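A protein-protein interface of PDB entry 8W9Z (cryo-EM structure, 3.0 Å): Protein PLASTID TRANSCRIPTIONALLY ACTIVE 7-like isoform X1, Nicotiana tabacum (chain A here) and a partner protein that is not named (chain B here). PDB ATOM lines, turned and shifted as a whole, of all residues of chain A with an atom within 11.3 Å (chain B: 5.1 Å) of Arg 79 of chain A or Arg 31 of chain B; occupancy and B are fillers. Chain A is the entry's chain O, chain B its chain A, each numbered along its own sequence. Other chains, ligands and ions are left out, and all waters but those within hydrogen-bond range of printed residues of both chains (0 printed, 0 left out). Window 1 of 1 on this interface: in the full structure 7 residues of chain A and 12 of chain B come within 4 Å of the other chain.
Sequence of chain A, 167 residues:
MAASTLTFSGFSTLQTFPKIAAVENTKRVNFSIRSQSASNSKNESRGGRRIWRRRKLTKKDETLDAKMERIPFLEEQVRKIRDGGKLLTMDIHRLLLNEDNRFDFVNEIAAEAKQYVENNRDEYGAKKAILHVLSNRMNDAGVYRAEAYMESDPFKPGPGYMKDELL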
ATOM      1  N   ILE A  71     -18.928  14.596  -2.388  1.00  0.00           N
ATOM      2  CA  ILE A  71     -17.964  14.343  -1.314  1.00  0.00           C
ATOM      3  C   ILE A  71     -18.605  13.411  -0.290  1.00  0.00           C
ATOM      4  O   ILE A  71     -19.733  13.675   0.156  1.00  0.00           O
ATOM      5  CB  ILE A  71     -17.515  15.654  -0.670  1.00  0.00           C
ATOM      6  CG1 ILE A  71     -16.273  16.210  -1.377  1.00  0.00           C
ATOM      7  CG2 ILE A  71     -17.213  15.459   0.812  1.00  0.00           C
ATOM      8  CD1 ILE A  71     -16.495  16.629  -2.814  1.00  0.00           C
ATOM      9  N   PRO A  72     -17.941  12.314   0.086  1.00  0.00           N
ATOM     10  CA  PRO A  72     -18.572  11.381   1.034  1.00  0.00           C
ATOM     11  C   PRO A  72     -18.714  11.949   2.433  1.00  0.00           C
ATOM     12  O   PRO A  72     -19.756  11.755   3.071  1.00  0.00           O
ATOM     13  CB  PRO A  72     -17.629  10.167   1.008  1.00  0.00           C
ATOM     14  CG  PRO A  72     -16.830  10.314  -0.254  1.00  0.00           C
ATOM     15  CD  PRO A  72     -16.680  11.786  -0.458  1.00  0.00           C
ATOM     16  N   PHE A  73     -17.695  12.649   2.933  1.00  0.00           N
ATOM     17  CA  PHE A  73     -17.680  13.133   4.312  1.00  0.00           C
ATOM     18  C   PHE A  73     -18.152  14.584   4.320  1.00  0.00           C
ATOM     19  O   PHE A  73     -17.372  15.525   4.463  1.00  0.00           O
ATOM     20  CB  PHE A  73     -16.287  12.982   4.911  1.00  0.00           C
ATOM     21  CG  PHE A  73     -15.540  11.783   4.403  1.00  0.00           C
ATOM     22  CD1 PHE A  73     -15.796  10.523   4.914  1.00  0.00           C
ATOM     23  CD2 PHE A  73     -14.583  11.917   3.412  1.00  0.00           C
ATOM     24  CE1 PHE A  73     -15.111   9.420   4.446  1.00  0.00           C
ATOM     25  CE2 PHE A  73     -13.895  10.817   2.942  1.00  0.00           C
ATOM     26  CZ  PHE A  73     -14.159   9.568   3.461  1.00  0.00           C
ATOM     27  N   LEU A  74     -19.464  14.758   4.164  1.00  0.00           N
ATOM     28  CA  LEU A  74     -20.050  16.089   4.142  1.00  0.00           C
ATOM     29  C   LEU A  74     -21.367  16.189   4.901  1.00  0.00           C
ATOM     30  O   LEU A  74     -21.974  17.264   4.902  1.00  0.00           O
ATOM     31  CB  LEU A  74     -20.257  16.548   2.689  1.00  0.00           C
ATOM     32  CG  LEU A  74     -20.244  18.053   2.429  1.00  0.00           C
ATOM     33  CD1 LEU A  74     -18.993  18.662   3.030  1.00  0.00           C
ATOM     34  CD2 LEU A  74     -20.327  18.345   0.940  1.00  0.00           C
ATOM     35  N   GLU A  75     -21.822  15.119   5.555  1.00  0.00           N
ATOM     36  CA  GLU A  75     -23.107  15.160   6.241  1.00  0.00           C
ATOM     37  C   GLU A  75     -23.033  15.915   7.563  1.00  0.00           C
ATOM     38  O   GLU A  75     -24.045  16.467   8.014  1.00  0.00           O
ATOM     39  CB  GLU A  75     -23.617  13.738   6.480  1.00  0.00           C
ATOM     40  CG  GLU A  75     -23.760  12.911   5.213  1.00  0.00           C
ATOM     41  CD  GLU A  75     -24.247  11.502   5.489  1.00  0.00           C
ATOM     42  OE1 GLU A  75     -24.462  11.166   6.673  1.00  0.00           O
ATOM     43  OE2 GLU A  75     -24.414  10.729   4.522  1.00  0.00           O
ATOM     44  N   GLU A  76     -21.853  15.957   8.187  1.00  0.00           N
ATOM     45  CA  GLU A  76     -21.723  16.599   9.491  1.00  0.00           C
ATOM     46  C   GLU A  76     -22.010  18.093   9.398  1.00  0.00           C
ATOM     47  O   GLU A  76     -22.789  18.637  10.190  1.00  0.00           O
ATOM     48  CB  GLU A  76     -20.325  16.345  10.059  1.00  0.00           C
ATOM     49  CG  GLU A  76     -20.177  16.655  11.545  1.00  0.00           C
ATOM     50  CD  GLU A  76     -19.915  18.122  11.824  1.00  0.00           C
ATOM     51  OE1 GLU A  76     -19.458  18.833  10.903  1.00  0.00           O
ATOM     52  OE2 GLU A  76     -20.165  18.566  12.964  1.00  0.00           O
ATOM     53  N   GLN A  77     -21.396  18.776   8.430  1.00  0.00           N
ATOM     54  CA  GLN A  77     -21.621  20.211   8.314  1.00  0.00           C
ATOM     55  C   GLN A  77     -23.021  20.520   7.800  1.00  0.00           C
ATOM     56  O   GLN A  77     -23.572  21.577   8.117  1.00  0.00           O
ATOM     57  CB  GLN A  77     -20.558  20.850   7.416  1.00  0.00           C
ATOM     58  CG  GLN A  77     -20.720  20.585   5.932  1.00  0.00           C
ATOM     59  CD  GLN A  77     -19.716  21.362   5.103  1.00  0.00           C
ATOM     60  OE1 GLN A  77     -18.618  21.667   5.566  1.00  0.00           O
ATOM     61  NE2 GLN A  77     -20.093  21.693   3.875  1.00  0.00           N
ATOM     62  N   VAL A  78     -23.626  19.606   7.038  1.00  0.00           N
ATOM     63  CA  VAL A  78     -25.014  19.794   6.623  1.00  0.00           C
ATOM     64  C   VAL A  78     -25.940  19.740   7.834  1.00  0.00           C
ATOM     65  O   VAL A  78     -26.839  20.578   7.990  1.00  0.00           O
ATOM     66  CB  VAL A  78     -25.405  18.750   5.562  1.00  0.00           C
ATOM     67  CG1 VAL A  78     -26.895  18.815   5.277  1.00  0.00           C
ATOM     68  CG2 VAL A  78     -24.613  18.974   4.286  1.00  0.00           C
ATOM     69  N   ARG A  79     -25.731  18.755   8.711  1.00  0.00           N
ATOM     70  CA  ARG A  79     -26.512  18.693   9.942  1.00  0.00           C
ATOM     71  C   ARG A  79     -26.254  19.915  10.816  1.00  0.00           C
ATOM     72  O   ARG A  79     -27.173  20.430  11.463  1.00  0.00           O
ATOM     73  CB  ARG A  79     -26.196  17.409  10.709  1.00  0.00           C
ATOM     74  CG  ARG A  79     -26.628  16.135  10.002  1.00  0.00           C
ATOM     75  CD  ARG A  79     -26.481  14.927  10.912  1.00  0.00           C
ATOM     76  NE  ARG A  79     -25.106  14.748  11.370  1.00  0.00           N
ATOM     77  CZ  ARG A  79     -24.214  13.970  10.766  1.00  0.00           C
ATOM     78  NH1 ARG A  79     -24.549  13.294   9.676  1.00  0.00           N
ATOM     79  NH2 ARG A  79     -22.984  13.868  11.253  1.00  0.00           N
ATOM     80  N   LYS A  80     -25.010  20.398  10.840  1.00  0.00           N
ATOM     81  CA  LYS A  80     -24.697  21.593  11.615  1.00  0.00           C
ATOM     82  C   LYS A  80     -25.432  22.813  11.071  1.00  0.00           C
ATOM     83  O   LYS A  80     -25.937  23.637  11.841  1.00  0.00           O
ATOM     84  CB  LYS A  80     -23.187  21.834  11.621  1.00  0.00           C
ATOM     85  CG  LYS A  80     -22.755  23.058  12.414  1.00  0.00           C
ATOM     86  CD  LYS A  80     -23.120  22.925  13.884  1.00  0.00           C
ATOM     87  CE  LYS A  80     -22.408  21.745  14.527  1.00  0.00           C
ATOM     88  NZ  LYS A  80     -22.759  21.601  15.967  1.00  0.00           N
ATOM     89  N   ILE A  81     -25.501  22.944   9.744  1.00  0.00           N
ATOM     90  CA  ILE A  81     -26.241  24.046   9.138  1.00  0.00           C
ATOM     91  C   ILE A  81     -27.723  23.940   9.472  1.00  0.00           C
ATOM     92  O   ILE A  81     -28.372  24.936   9.815  1.00  0.00           O
ATOM     93  CB  ILE A  81     -26.010  24.075   7.615  1.00  0.00           C
ATOM     94  CG1 ILE A  81     -24.568  24.469   7.295  1.00  0.00           C
ATOM     95  CG2 ILE A  81     -26.979  25.034   6.941  1.00  0.00           C
ATOM     96  CD1 ILE A  81     -24.268  24.492   5.815  1.00  0.00           C
ATOM     97  N   ARG A  82     -28.281  22.729   9.387  1.00  0.00           N
ATOM     98  CA  ARG A  82     -29.710  22.571   9.639  1.00  0.00           C
ATOM     99  C   ARG A  82     -30.057  22.765  11.112  1.00  0.00           C
ATOM    100  O   ARG A  82     -31.186  23.153  11.432  1.00  0.00           O
ATOM    101  CB  ARG A  82     -30.188  21.199   9.165  1.00  0.00           C
ATOM    102  CG  ARG A  82     -30.099  20.989   7.663  1.00  0.00           C
ATOM    103  CD  ARG A  82     -31.133  19.979   7.194  1.00  0.00           C
ATOM    104  NE  ARG A  82     -31.095  18.748   7.979  1.00  0.00           N
ATOM    105  CZ  ARG A  82     -30.442  17.649   7.619  1.00  0.00           C
ATOM    106  NH1 ARG A  82     -29.768  17.620   6.478  1.00  0.00           N
ATOM    107  NH2 ARG A  82     -30.464  16.576   8.399  1.00  0.00           N
ATOM    108  N   ASP A  83     -29.114  22.506  12.017  1.00  0.00           N
ATOM    109  CA  ASP A  83     -29.407  22.576  13.444  1.00  0.00           C
ATOM    110  C   ASP A  83     -29.108  23.953  14.034  1.00  0.00           C
ATOM    111  O   ASP A  83     -29.932  24.503  14.770  1.00  0.00           O
ATOM    112  CB  ASP A  83     -28.615  21.499  14.192  1.00  0.00           C
ATOM    113  CG  ASP A  83     -29.085  21.314  15.623  1.00  0.00           C
ATOM    114  OD1 ASP A  83     -30.137  21.879  15.986  1.00  0.00           O
ATOM    115  OD2 ASP A  83     -28.399  20.601  16.386  1.00  0.00           O
ATOM    116  N   GLY A  84     -27.936  24.515  13.729  1.00  0.00           N
ATOM    117  CA  GLY A  84     -27.556  25.788  14.319  1.00  0.00           C
ATOM    118  C   GLY A  84     -28.469  26.933  13.928  1.00  0.00           C
ATOM    119  O   GLY A  84     -28.640  27.884  14.695  1.00  0.00           O
ATOM    120  N   GLY A  85     -29.066  26.862  12.742  1.00  0.00           N
ATOM    121  CA  GLY A  85     -29.984  27.893  12.305  1.00  0.00           C
ATOM    122  C   GLY A  85     -29.432  28.762  11.195  1.00  0.00           C
ATOM    123  O   GLY A  85     -29.782  29.942  11.090  1.00  0.00           O
ATOM    124  N   LYS A  86     -28.566  28.193  10.360  1.00  0.00           N
ATOM    125  CA  LYS A  86     -28.028  28.910   9.213  1.00  0.00           C
ATOM    126  C   LYS A  86     -28.961  28.888   8.012  1.00  0.00           C
ATOM    127  O   LYS A  86     -28.681  29.569   7.019  1.00  0.00           O
ATOM    128  CB  LYS A  86     -26.667  28.330   8.815  1.00  0.00           C
ATOM    129  CG  LYS A  86     -25.596  28.471   9.885  1.00  0.00           C
ATOM    130  CD  LYS A  86     -24.255  27.949   9.399  1.00  0.00           C
ATOM    131  CE  LYS A  86     -23.766  28.727   8.190  1.00  0.00           C
ATOM    132  NZ  LYS A  86     -23.587  30.173   8.496  1.00  0.00           N
ATOM    133  N   LEU A  87     -30.056  28.126   8.075  1.00  0.00           N
ATOM    134  CA  LEU A  87     -31.017  28.116   6.978  1.00  0.00           C
ATOM    135  C   LEU A  87     -31.720  29.459   6.837  1.00  0.00           C
ATOM    136  O   LEU A  87     -32.033  29.880   5.716  1.00  0.00           O
ATOM    137  CB  LEU A  87     -32.045  27.006   7.190  1.00  0.00           C
ATOM    138  CG  LEU A  87     -31.519  25.589   7.427  1.00  0.00           C
ATOM    139  CD1 LEU A  87     -32.670  24.634   7.698  1.00  0.00           C
ATOM    140  CD2 LEU A  87     -30.693  25.112   6.247  1.00  0.00           C
ATOM    141  N   MET A  90     -29.760  32.006   4.850  1.00  0.00           N
ATOM    142  CA  MET A  90     -29.856  31.790   3.412  1.00  0.00           C
ATOM    143  C   MET A  90     -31.226  32.190   2.882  1.00  0.00           C
ATOM    144  O   MET A  90     -31.332  32.750   1.785  1.00  0.00           O
ATOM    145  CB  MET A  90     -29.575  30.327   3.076  1.00  0.00           C
ATOM    146  CG  MET A  90     -28.414  29.722   3.837  1.00  0.00           C
ATOM    147  SD  MET A  90     -28.127  28.005   3.368  1.00  0.00           S
ATOM    148  CE  MET A  90     -29.781  27.340   3.531  1.00  0.00           C
ATOM    149  N   GLU A 151     -36.764  22.877  15.243  1.00  0.00           N
ATOM    150  CA  GLU A 151     -36.471  21.444  15.182  1.00  0.00           C
ATOM    151  C   GLU A 151     -35.712  21.080  16.454  1.00  0.00           C
ATOM    152  O   GLU A 151     -34.514  21.354  16.567  1.00  0.00           O
ATOM    153  CB  GLU A 151     -35.671  21.089  13.933  1.00  0.00           C
ATOM    154  CG  GLU A 151     -36.459  21.177  12.635  1.00  0.00           C
ATOM    155  CD  GLU A 151     -37.516  20.094  12.516  1.00  0.00           C
ATOM    156  OE1 GLU A 151     -37.401  19.065  13.214  1.00  0.00           O
ATOM    157  OE2 GLU A 151     -38.464  20.272  11.721  1.00  0.00           O
ATOM    158  N   SER A 152     -36.412  20.467  17.404  1.00  0.00           N
ATOM    159  CA  SER A 152     -35.793  20.091  18.664  1.00  0.00           C
ATOM    160  C   SER A 152     -34.813  18.940  18.459  1.00  0.00           C
ATOM    161  O   SER A 152     -34.840  18.232  17.449  1.00  0.00           O
ATOM    162  CB  SER A 152     -36.857  19.701  19.690  1.00  0.00           C
ATOM    163  OG  SER A 152     -37.742  20.778  19.942  1.00  0.00           O
ATOM    164  N   ASP A 153     -33.933  18.758  19.445  1.00  0.00           N
ATOM    165  CA  ASP A 153     -32.930  17.704  19.391  1.00  0.00           C
ATOM    166  C   ASP A 153     -33.513  16.421  19.968  1.00  0.00           C
ATOM    167  O   ASP A 153     -33.824  16.380  21.168  1.00  0.00           O
ATOM    168  CB  ASP A 153     -31.679  18.114  20.157  1.00  0.00           C
ATOM    169  CG  ASP A 153     -31.996  18.782  21.483  1.00  0.00           C
ATOM    170  OD1 ASP A 153     -33.185  19.069  21.737  1.00  0.00           O
ATOM    171  OD2 ASP A 153     -31.056  19.017  22.269  1.00  0.00           O
ATOM    172  N   PRO A 154     -33.684  15.361  19.170  1.00  0.00           N
ATOM    173  CA  PRO A 154     -34.223  14.106  19.717  1.00  0.00           C
ATOM    174  C   PRO A 154     -33.259  13.372  20.633  1.00  0.00           C
ATOM    175  O   PRO A 154     -33.657  12.372  21.244  1.00  0.00           O
ATOM    176  CB  PRO A 154     -34.528  13.274  18.462  1.00  0.00           C
ATOM    177  CG  PRO A 154     -34.505  14.252  17.317  1.00  0.00           C
ATOM    178  CD  PRO A 154     -33.515  15.297  17.711  1.00  0.00           C
ATOM    179  N   PHE A 155     -32.010  13.829  20.749  1.00  0.00           N
ATOM    180  CA  PHE A 155     -30.997  13.168  21.559  1.00  0.00           C
ATOM    181  C   PHE A 155     -30.740  13.897  22.874  1.00  0.00           C
ATOM    182  O   PHE A 155     -29.603  13.925  23.357  1.00  0.00           O
ATOM    183  CB  PHE A 155     -29.697  13.029  20.767  1.00  0.00           C
ATOM    184  CG  PHE A 155     -29.863  12.325  19.449  1.00  0.00           C
ATOM    185  CD1 PHE A 155     -30.774  11.292  19.307  1.00  0.00           C
ATOM    186  CD2 PHE A 155     -29.110  12.703  18.349  1.00  0.00           C
ATOM    187  CE1 PHE A 155     -30.928  10.646  18.095  1.00  0.00           C
ATOM    188  CE2 PHE A 155     -29.259  12.062  17.135  1.00  0.00           C
ATOM    189  CZ  PHE A 155     -30.170  11.032  17.008  1.00  0.00           C
ATOM    190  N   LYS A 156     -31.778  14.489  23.464  1.00  0.00           N
ATOM    191  CA  LYS A 156     -31.635  15.213  24.717  1.00  0.00           C
ATOM    192  C   LYS A 156     -32.215  14.380  25.847  1.00  0.00           C
ATOM    193  O   LYS A 156     -33.445  14.229  25.923  1.00  0.00           O
ATOM    194  CB  LYS A 156     -32.337  16.568  24.639  1.00  0.00           C
ATOM    195  N   LYS B  16     -26.717   2.852  20.493  1.00  0.00           N
ATOM    196  CA  LYS B  16     -27.702   2.750  19.427  1.00  0.00           C
ATOM    197  C   LYS B  16     -27.100   3.243  18.120  1.00  0.00           C
ATOM    198  O   LYS B  16     -26.208   4.095  18.112  1.00  0.00           O
ATOM    199  CB  LYS B  16     -28.965   3.561  19.746  1.00  0.00           C
ATOM    200  CG  LYS B  16     -29.701   3.114  20.996  1.00  0.00           C
ATOM    201  CD  LYS B  16     -30.887   4.019  21.287  1.00  0.00           C
ATOM    202  CE  LYS B  16     -31.844   4.075  20.107  1.00  0.00           C
ATOM    203  NZ  LYS B  16     -32.370   2.728  19.754  1.00  0.00           N
ATOM    204  N   CYS B  17     -27.601   2.699  17.014  1.00  0.00           N
ATOM    205  CA  CYS B  17     -27.214   3.131  15.672  1.00  0.00           C
ATOM    206  C   CYS B  17     -28.327   4.027  15.139  1.00  0.00           C
ATOM    207  O   CYS B  17     -29.371   3.542  14.697  1.00  0.00           O
ATOM    208  CB  CYS B  17     -26.970   1.933  14.761  1.00  0.00           C
ATOM    209  SG  CYS B  17     -26.521   2.369  13.066  1.00  0.00           S
ATOM    210  N   VAL B  18     -28.100   5.338  15.182  1.00  0.00           N
ATOM    211  CA  VAL B  18     -29.149   6.286  14.820  1.00  0.00           C
ATOM    212  C   VAL B  18     -29.253   6.437  13.307  1.00  0.00           C
ATOM    213  O   VAL B  18     -30.355   6.454  12.747  1.00  0.00           O
ATOM    214  CB  VAL B  18     -28.910   7.640  15.516  1.00  0.00           C
ATOM    215  CG1 VAL B  18     -29.289   7.544  16.981  1.00  0.00           C
ATOM    216  CG2 VAL B  18     -27.461   8.068  15.374  1.00  0.00           C
ATOM    217  N   GLU B  19     -28.119   6.551  12.621  1.00  0.00           N
ATOM    218  CA  GLU B  19     -28.096   6.740  11.179  1.00  0.00           C
ATOM    219  C   GLU B  19     -27.291   5.630  10.518  1.00  0.00           C
ATOM    220  O   GLU B  19     -26.257   5.205  11.040  1.00  0.00           O
ATOM    221  CB  GLU B  19     -27.508   8.105  10.809  1.00  0.00           C
ATOM    222  CG  GLU B  19     -28.222   9.299  11.437  1.00  0.00           C
ATOM    223  CD  GLU B  19     -29.540   9.637  10.758  1.00  0.00           C
ATOM    224  OE1 GLU B  19     -30.416   8.752  10.654  1.00  0.00           O
ATOM    225  OE2 GLU B  19     -29.700  10.797  10.323  1.00  0.00           O
ATOM    226  N   TYR B  29     -21.805   4.129   5.865  1.00  0.00           N
ATOM    227  CA  TYR B  29     -21.882   5.185   6.861  1.00  0.00           C
ATOM    228  C   TYR B  29     -22.590   4.657   8.100  1.00  0.00           C
ATOM    229  O   TYR B  29     -23.481   3.809   8.009  1.00  0.00           O
ATOM    230  CB  TYR B  29     -22.610   6.421   6.320  1.00  0.00           C
ATOM    231  CG  TYR B  29     -22.757   7.540   7.324  1.00  0.00           C
ATOM    232  CD1 TYR B  29     -21.708   8.411   7.578  1.00  0.00           C
ATOM    233  CD2 TYR B  29     -23.946   7.730   8.013  1.00  0.00           C
ATOM    234  CE1 TYR B  29     -21.836   9.437   8.491  1.00  0.00           C
ATOM    235  CE2 TYR B  29     -24.084   8.754   8.930  1.00  0.00           C
ATOM    236  CZ  TYR B  29     -23.026   9.603   9.164  1.00  0.00           C
ATOM    237  OH  TYR B  29     -23.157  10.625  10.076  1.00  0.00           O
ATOM    238  N   GLY B  30     -22.184   5.171   9.257  1.00  0.00           N
ATOM    239  CA  GLY B  30     -22.800   4.795  10.514  1.00  0.00           C
ATOM    240  C   GLY B  30     -22.646   5.854  11.584  1.00  0.00           C
ATOM    241  O   GLY B  30     -21.576   6.451  11.726  1.00  0.00           O
ATOM    242  N   ARG B  31     -23.710   6.098  12.346  1.00  0.00           N
ATOM    243  CA  ARG B  31     -23.695   7.068  13.433  1.00  0.00           C
ATOM    244  C   ARG B  31     -24.191   6.383  14.696  1.00  0.00           C
ATOM    245  O   ARG B  31     -25.240   5.732  14.679  1.00  0.00           O
ATOM    246  CB  ARG B  31     -24.561   8.285  13.098  1.00  0.00           C
ATOM    247  CG  ARG B  31     -24.292   9.506  13.956  1.00  0.00           C
ATOM    248  CD  ARG B  31     -25.035  10.717  13.413  1.00  0.00           C
ATOM    249  NE  ARG B  31     -24.669  11.946  14.107  1.00  0.00           N
ATOM    250  CZ  ARG B  31     -25.316  12.430  15.161  1.00  0.00           C
ATOM    251  NH1 ARG B  31     -26.368  11.786  15.649  1.00  0.00           N
ATOM    252  NH2 ARG B  31     -24.912  13.558  15.729  1.00  0.00           N
ATOM    253  N   PHE B  32     -23.440   6.526  15.784  1.00  0.00           N
ATOM    254  CA  PHE B  32     -23.726   5.820  17.023  1.00  0.00           C
ATOM    255  C   PHE B  32     -23.776   6.803  18.185  1.00  0.00           C
ATOM    256  O   PHE B  32     -23.267   7.923  18.102  1.00  0.00           O
ATOM    257  CB  PHE B  32     -22.687   4.726  17.290  1.00  0.00           C
ATOM    258  CG  PHE B  32     -22.588   3.710  16.189  1.00  0.00           C
ATOM    259  CD1 PHE B  32     -23.393   2.585  16.193  1.00  0.00           C
ATOM    260  CD2 PHE B  32     -21.696   3.884  15.146  1.00  0.00           C
ATOM    261  CE1 PHE B  32     -23.307   1.651  15.181  1.00  0.00           C
ATOM    262  CE2 PHE B  32     -21.606   2.953  14.130  1.00  0.00           C
ATOM    263  CZ  PHE B  32     -22.412   1.835  14.149  1.00  0.00           C
ATOM    264  N   ILE B  33     -24.399   6.365  19.277  1.00  0.00           N
ATOM    265  CA  ILE B  33     -24.649   7.210  20.438  1.00  0.00           C
ATOM    266  C   ILE B  33     -24.396   6.403  21.704  1.00  0.00           C
ATOM    267  O   ILE B  33     -24.897   5.283  21.842  1.00  0.00           O
ATOM    268  CB  ILE B  33     -26.088   7.769  20.432  1.00  0.00           C
ATOM    269  CG1 ILE B  33     -26.210   8.927  19.442  1.00  0.00           C
ATOM    270  CG2 ILE B  33     -26.514   8.195  21.828  1.00  0.00           C
ATOM    271  CD1 ILE B  33     -27.571   9.585  19.446  1.00  0.00           C
ATOM    272  N   PHE B 200     -20.751  10.692  19.986  1.00  0.00           N
ATOM    273  CA  PHE B 200     -21.300  10.505  18.643  1.00  0.00           C
ATOM    274  C   PHE B 200     -20.178  10.016  17.731  1.00  0.00           C
ATOM    275  O   PHE B 200     -19.349  10.812  17.282  1.00  0.00           O
ATOM    276  CB  PHE B 200     -21.912  11.796  18.111  1.00  0.00           C
ATOM    277  CG  PHE B 200     -23.100  12.277  18.895  1.00  0.00           C
ATOM    278  CD1 PHE B 200     -22.931  13.051  20.029  1.00  0.00           C
ATOM    279  CD2 PHE B 200     -24.385  11.964  18.490  1.00  0.00           C
ATOM    280  CE1 PHE B 200     -24.022  13.495  20.749  1.00  0.00           C
ATOM    281  CE2 PHE B 200     -25.478  12.407  19.203  1.00  0.00           C
ATOM    282  CZ  PHE B 200     -25.297  13.173  20.335  1.00  0.00           C
ATOM    283  N   LEU B 201     -20.156   8.716  17.450  1.00  0.00           N
ATOM    284  CA  LEU B 201     -19.134   8.114  16.603  1.00  0.00           C
ATOM    285  C   LEU B 201     -19.639   8.003  15.171  1.00  0.00           C
ATOM    286  O   LEU B 201     -20.761   7.540  14.936  1.00  0.00           O
ATOM    287  CB  LEU B 201     -18.736   6.734  17.126  1.00  0.00           C
ATOM    288  CG  LEU B 201     -17.933   6.690  18.425  1.00  0.00           C
ATOM    289  CD1 LEU B 201     -17.676   5.252  18.839  1.00  0.00           C
ATOM    290  CD2 LEU B 201     -16.625   7.446  18.267  1.00  0.00           C
ATOM    291  N   GLU B 202     -18.811   8.428  14.220  1.00  0.00           N
ATOM    292  CA  GLU B 202     -19.096   8.305  12.797  1.00  0.00           C
ATOM    293  C   GLU B 202     -18.024   7.439  12.152  1.00  0.00           C
ATOM    294  O   GLU B 202     -16.828   7.682  12.346  1.00  0.00           O
ATOM    295  CB  GLU B 202     -19.147   9.675  12.115  1.00  0.00           C
ATOM    296  CG  GLU B 202     -20.380  10.511  12.433  1.00  0.00           C
ATOM    297  CD  GLU B 202     -20.318  11.166  13.799  1.00  0.00           C
ATOM    298  OE1 GLU B 202     -20.943  10.640  14.743  1.00  0.00           O
ATOM    299  OE2 GLU B 202     -19.644  12.210  13.929  1.00  0.00           O
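The guanidinium group (NH1) of Arg 79 of chain A is in hydrogen-bond range of the side-chain hydroxyl (OH) of Tyr 29 of chain B, at 3.0 Å.
The backbone carbonyl oxygen (O) of Lys 16 of chain B sits at hydrogen-bond distance from the backbone NH (N) of Ile 33 of chain B, 3.1 Å away.
The backbone NH (N) of Val 18 of chain B is in hydrogen-bond range of the backbone carbonyl oxygen (O) of Arg 31 of chain B (2.9 Å).
O of Glu 19 of chain B lies within hydrogen-bond range of N of Arg 31 of chain B.
NE of Arg 31 of chain B lies within salt-bridge range of OE1 of Glu 202 of chain B (3.999 Å).
The guanidinium group (NH1) of Arg 79 of chain A is in salt-bridge range of the side-chain carboxylate (OE1) of Glu 75 of chain A, 3.7 Å away.
Printed residues of chain B that touch a printed residue of chain A: Val 18, Tyr 29, Arg 31, Ile 33 and Phe 200.
Along chain B the printed residues that touch a printed residue of chain A span positions 18 to 200.
Of the 24 printed residues of chain A, 3 touch a printed residue of chain B.
Hydrophobic or aromatic side chains of chain A within 4 Å of the printed part of chain B: Phe 155.
Among the printed residues, no Asp or Glu carboxylate lies within 4 Å of a Lys or Arg side-chain nitrogen of the other chain.
Printed residues of chain B within 4 Å of Glu 75 of chain A: Tyr 29.
Of chain B, only Tyr 29 and Arg 31 come within 4 Å of Arg 79 of chain A.
Ile 81 of chain A touches none of the printed residues of chain B.
Of the printed residues of chain B, Phe 155 of chain A touches Val 18, Arg 31, Ile 33 and Phe 200.
Tyr 29 of chain B touches just these residues of chain A: Glu 75 and Arg 79.
Gly 30 of chain B touches none of the printed residues of chain A.
No residue of chain A comes within 4 Å of Phe 32 of chain B.
Ile 33 of chain B touches one residue of chain A.
Phe 200 of chain B touches one residue of chain A.
The nearest residue of chain A that does not touch Arg 31 of chain B is Glu 75 of chain A (6.8 Å).
The nearest printed residue of chain B that does not touch Glu 75 of chain A is Glu 19 of chain B (6.0 Å).
OE1 of Glu 75 of chain A touches CZ of Tyr 29 of chain B (3.3 Å).
NH2 of Arg 79 of chain A touches NE of Arg 31 of chain B (3.8 Å).
Phe 155 of chain A touches Val 18 of chain B.
CE2 of Phe 155 of chain A touches NH1 of Arg 31 of chain B (3.3 Å).
CG of Phe 155 of chain A touches CD1 of Ile 33 of chain B (3.6 Å).
CD2 of Phe 155 of chain A touches CE2 of Phe 200 of chain B, 3.7 Å away.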
